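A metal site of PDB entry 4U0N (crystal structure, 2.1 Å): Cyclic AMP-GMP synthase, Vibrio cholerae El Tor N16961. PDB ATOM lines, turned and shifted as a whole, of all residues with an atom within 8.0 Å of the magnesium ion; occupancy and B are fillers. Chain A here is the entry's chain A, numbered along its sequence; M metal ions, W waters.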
ATOM      1  N   GLN A 116     -20.462  15.155  17.474  1.00  0.00           N
ATOM      2  CA  GLN A 116     -19.951  13.982  18.169  1.00  0.00           C
ATOM      3  C   GLN A 116     -19.853  14.177  19.686  1.00  0.00           C
ATOM      4  O   GLN A 116     -18.821  13.895  20.292  1.00  0.00           O
ATOM      5  CB  GLN A 116     -18.583  13.548  17.606  1.00  0.00           C
ATOM      6  CG  GLN A 116     -18.659  13.010  16.187  1.00  0.00           C
ATOM      7  CD  GLN A 116     -17.295  12.579  15.640  1.00  0.00           C
ATOM      8  OE1 GLN A 116     -16.307  12.513  16.372  1.00  0.00           O
ATOM      9  NE2 GLN A 116     -17.251  12.284  14.343  1.00  0.00           N
ATOM     10  N   MET A 130     -14.144  13.658   8.678  1.00  0.00           N
ATOM     11  CA  MET A 130     -14.991  13.917   9.838  1.00  0.00           C
ATOM     12  C   MET A 130     -16.410  13.397   9.588  1.00  0.00           C
ATOM     13  O   MET A 130     -17.008  13.689   8.545  1.00  0.00           O
ATOM     14  CB  MET A 130     -14.992  15.409  10.176  1.00  0.00           C
ATOM     15  CG  MET A 130     -13.619  15.970  10.541  1.00  0.00           C
ATOM     16  SD  MET A 130     -13.631  17.697  11.057  1.00  0.00           S
ATOM     17  CE  MET A 130     -13.662  18.553   9.494  1.00  0.00           C
ATOM     18  N   ASP A 131     -16.926  12.603  10.531  1.00  0.00           N
ATOM     19  CA  ASP A 131     -18.276  12.039  10.435  1.00  0.00           C
ATOM     20  C   ASP A 131     -19.280  12.931  11.172  1.00  0.00           C
ATOM     21  O   ASP A 131     -19.365  12.896  12.407  1.00  0.00           O
ATOM     22  CB  ASP A 131     -18.285  10.619  10.998  1.00  0.00           C
ATOM     23  CG  ASP A 131     -19.690  10.056  11.200  1.00  0.00           C
ATOM     24  OD1 ASP A 131     -20.507  10.043  10.237  1.00  0.00           O
ATOM     25  OD2 ASP A 131     -19.990   9.618  12.334  1.00  0.00           O
ATOM     26  N   ILE A 132     -20.027  13.716  10.410  1.00  0.00           N
ATOM     27  CA  ILE A 132     -21.032  14.620  10.972  1.00  0.00           C
ATOM     28  C   ILE A 132     -22.440  14.119  10.686  1.00  0.00           C
ATOM     29  O   ILE A 132     -22.782  13.818   9.538  1.00  0.00           O
ATOM     30  CB  ILE A 132     -20.886  16.044  10.385  1.00  0.00           C
ATOM     31  CG1 ILE A 132     -19.473  16.586  10.636  1.00  0.00           C
ATOM     32  CG2 ILE A 132     -21.936  16.981  10.968  1.00  0.00           C
ATOM     33  CD1 ILE A 132     -19.054  16.570  12.094  1.00  0.00           C
ATOM     34  N   ASP A 133     -23.259  14.042  11.735  1.00  0.00           N
ATOM     35  CA  ASP A 133     -24.649  13.613  11.592  1.00  0.00           C
ATOM     36  C   ASP A 133     -25.589  14.772  11.927  1.00  0.00           C
ATOM     37  O   ASP A 133     -25.493  15.353  13.003  1.00  0.00           O
ATOM     38  CB  ASP A 133     -24.951  12.432  12.508  1.00  0.00           C
ATOM     39  CG  ASP A 133     -24.189  11.178  12.112  1.00  0.00           C
ATOM     40  OD1 ASP A 133     -23.753  11.084  10.944  1.00  0.00           O
ATOM     41  OD2 ASP A 133     -24.032  10.274  12.970  1.00  0.00           O
ATOM     42  N   ASP A 134     -26.497  15.090  10.996  1.00  0.00           N
ATOM     43  CA  ASP A 134     -27.572  16.041  11.290  1.00  0.00           C
ATOM     44  C   ASP A 134     -28.909  15.473  10.833  1.00  0.00           C
ATOM     45  O   ASP A 134     -29.204  15.428   9.627  1.00  0.00           O
ATOM     46  CB  ASP A 134     -27.318  17.403  10.653  1.00  0.00           C
ATOM     47  CG  ASP A 134     -28.248  18.481  11.188  1.00  0.00           C
ATOM     48  OD1 ASP A 134     -28.524  18.482  12.411  1.00  0.00           O
ATOM     49  OD2 ASP A 134     -28.725  19.323  10.394  1.00  0.00           O
ATOM     50  N   LYS A 177     -27.138   5.472   1.994  1.00  0.00           N
ATOM     51  CA  LYS A 177     -26.769   4.444   2.947  1.00  0.00           C
ATOM     52  C   LYS A 177     -28.010   3.814   3.566  1.00  0.00           C
ATOM     53  O   LYS A 177     -29.131   4.219   3.263  1.00  0.00           O
ATOM     54  CB  LYS A 177     -25.851   5.015   4.034  1.00  0.00           C
ATOM     55  CG  LYS A 177     -24.595   5.702   3.499  1.00  0.00           C
ATOM     56  CD  LYS A 177     -23.559   5.868   4.589  1.00  0.00           C
ATOM     57  CE  LYS A 177     -23.033   4.512   5.052  1.00  0.00           C
ATOM     58  NZ  LYS A 177     -22.334   3.790   3.953  1.00  0.00           N
ATOM     59  N   THR A 179     -29.135   3.825   6.799  1.00  0.00           N
ATOM     60  CA  THR A 179     -29.855   4.706   7.721  1.00  0.00           C
ATOM     61  C   THR A 179     -29.917   6.175   7.320  1.00  0.00           C
ATOM     62  O   THR A 179     -30.509   6.982   8.042  1.00  0.00           O
ATOM     63  CB  THR A 179     -29.269   4.628   9.154  1.00  0.00           C
ATOM     64  OG1 THR A 179     -28.023   5.341   9.199  1.00  0.00           O
ATOM     65  CG2 THR A 179     -29.038   3.182   9.559  1.00  0.00           C
ATOM     66  N   CYS A 180     -29.299   6.544   6.201  1.00  0.00           N
ATOM     67  CA  CYS A 180     -29.220   7.961   5.863  1.00  0.00           C
ATOM     68  C   CYS A 180     -28.766   8.236   4.440  1.00  0.00           C
ATOM     69  O   CYS A 180     -28.207   7.356   3.770  1.00  0.00           O
ATOM     70  CB  CYS A 180     -28.252   8.655   6.823  1.00  0.00           C
ATOM     71  SG  CYS A 180     -26.539   8.100   6.659  1.00  0.00           S
ATOM     72  N   GLY A 181     -29.020   9.453   3.975  1.00  0.00           N
ATOM     73  CA  GLY A 181     -28.405   9.948   2.764  1.00  0.00           C
ATOM     74  C   GLY A 181     -27.153  10.686   3.195  1.00  0.00           C
ATOM     75  O   GLY A 181     -27.142  11.322   4.250  1.00  0.00           O
ATOM     76  N   ARG A 182     -26.087  10.576   2.408  1.00  0.00           N
ATOM     77  CA  ARG A 182     -24.816  11.159   2.813  1.00  0.00           C
ATOM     78  C   ARG A 182     -24.273  12.128   1.773  1.00  0.00           C
ATOM     79  O   ARG A 182     -24.287  11.840   0.569  1.00  0.00           O
ATOM     80  CB  ARG A 182     -23.793  10.053   3.074  1.00  0.00           C
ATOM     81  CG  ARG A 182     -22.370  10.572   3.241  1.00  0.00           C
ATOM     82  CD  ARG A 182     -21.415   9.452   3.657  1.00  0.00           C
ATOM     83  NE  ARG A 182     -21.670   9.004   5.030  1.00  0.00           N
ATOM     84  CZ  ARG A 182     -20.986   8.038   5.637  1.00  0.00           C
ATOM     85  NH1 ARG A 182     -19.999   7.421   4.999  1.00  0.00           N
ATOM     86  NH2 ARG A 182     -21.280   7.700   6.884  1.00  0.00           N
ATOM     87  N   HIS A 191     -17.864  14.493   5.575  1.00  0.00           N
ATOM     88  CA  HIS A 191     -19.136  14.009   5.065  1.00  0.00           C
ATOM     89  C   HIS A 191     -20.188  14.227   6.144  1.00  0.00           C
ATOM     90  O   HIS A 191     -19.897  14.151   7.344  1.00  0.00           O
ATOM     91  CB  HIS A 191     -19.066  12.537   4.626  1.00  0.00           C
ATOM     92  CG  HIS A 191     -18.799  11.574   5.732  1.00  0.00           C
ATOM     93  ND1 HIS A 191     -17.594  10.933   5.886  1.00  0.00           N
ATOM     94  CD2 HIS A 191     -19.602  11.115   6.734  1.00  0.00           C
ATOM     95  CE1 HIS A 191     -17.642  10.134   6.945  1.00  0.00           C
ATOM     96  NE2 HIS A 191     -18.861  10.228   7.473  1.00  0.00           N
ATOM     97  N   ILE A 192     -21.405  14.528   5.709  1.00  0.00           N
ATOM     98  CA  ILE A 192     -22.501  14.755   6.639  1.00  0.00           C
ATOM     99  C   ILE A 192     -23.661  13.806   6.314  1.00  0.00           C
ATOM    100  O   ILE A 192     -24.163  13.764   5.180  1.00  0.00           O
ATOM    101  CB  ILE A 192     -22.960  16.231   6.621  1.00  0.00           C
ATOM    102  CG1 ILE A 192     -24.262  16.401   7.412  1.00  0.00           C
ATOM    103  CG2 ILE A 192     -23.127  16.728   5.200  1.00  0.00           C
ATOM    104  CD1 ILE A 192     -24.580  17.847   7.741  1.00  0.00           C
ATOM    105  N   ASP A 193     -24.045  13.028   7.319  1.00  0.00           N
ATOM    106  CA  ASP A 193     -25.122  12.060   7.165  1.00  0.00           C
ATOM    107  C   ASP A 193     -26.444  12.699   7.594  1.00  0.00           C
ATOM    108  O   ASP A 193     -26.502  13.359   8.642  1.00  0.00           O
ATOM    109  CB  ASP A 193     -24.842  10.809   8.000  1.00  0.00           C
ATOM    110  CG  ASP A 193     -23.579  10.090   7.569  1.00  0.00           C
ATOM    111  OD1 ASP A 193     -23.293  10.072   6.356  1.00  0.00           O
ATOM    112  OD2 ASP A 193     -22.856   9.550   8.444  1.00  0.00           O
ATOM    113  N   VAL A 194     -27.478  12.509   6.789  1.00  0.00           N
ATOM    114  CA  VAL A 194     -28.795  13.032   7.117  1.00  0.00           C
ATOM    115  C   VAL A 194     -29.797  11.897   7.310  1.00  0.00           C
ATOM    116  O   VAL A 194     -30.524  11.552   6.381  1.00  0.00           O
ATOM    117  CB  VAL A 194     -29.316  13.990   6.034  1.00  0.00           C
ATOM    118  CG1 VAL A 194     -30.699  14.535   6.404  1.00  0.00           C
ATOM    119  CG2 VAL A 194     -28.343  15.147   5.820  1.00  0.00           C
ATOM    120  N   PRO A 195     -29.829  11.304   8.515  1.00  0.00           N
ATOM    121  CA  PRO A 195     -30.869  10.319   8.808  1.00  0.00           C
ATOM    122  C   PRO A 195     -32.219  11.019   8.923  1.00  0.00           C
ATOM    123  O   PRO A 195     -32.260  12.225   9.182  1.00  0.00           O
ATOM    124  CB  PRO A 195     -30.447   9.764  10.174  1.00  0.00           C
ATOM    125  CG  PRO A 195     -29.673  10.880  10.812  1.00  0.00           C
ATOM    126  CD  PRO A 195     -28.932  11.537   9.666  1.00  0.00           C
HETATM  127 MG    MG M   1     -22.676   9.385  10.505  1.00  0.00          MG
HETATM  128  O   HOH W   1     -23.993   7.833  10.032  1.00  0.00           O
HETATM  129  O   HOH W   2     -21.682   7.608   9.952  1.00  0.00           O
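The side-chain carboxylate (OD1) of Asp 193 lies within salt-bridge range of the guanidinium group (NH2) of Arg 182 (3.2 Å). N of Asp 193 sits at hydrogen-bond distance from O of Ile 132 (2.7 Å). N of Asp 134 lies within hydrogen-bond range of O of Asp 193, 2.9 Å away. The side-chain carboxylate of Asp 131 lies close to a ring nitrogen (NE2) of His 191, 3.2 Å away. O of Asp 131 lies within hydrogen-bond range of NE2 of Gln 116, 2.9 Å away.
The magnesium ion is bound by the side-chain carboxylate (OD1) of Asp 133, at 2.1 Å. OD2 of Asp 193 is bound to the magnesium ion (2.1 Å). Water W1 is bound to the magnesium ion (2.1 Å). Water W2 is bound to the magnesium ion (2.1 Å). The magnesium ion is bound by the side-chain carboxylate (OD1) of Asp 131, 2.3 Å away. The magnesium ion has five donor atoms within binding distance.
Three residues have an atom within 4 Å of the magnesium ion: Asp 131, Asp 133 and Asp 193. The nearest printed residue that does not touch the magnesium ion is Arg 182 (4.2 Å).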
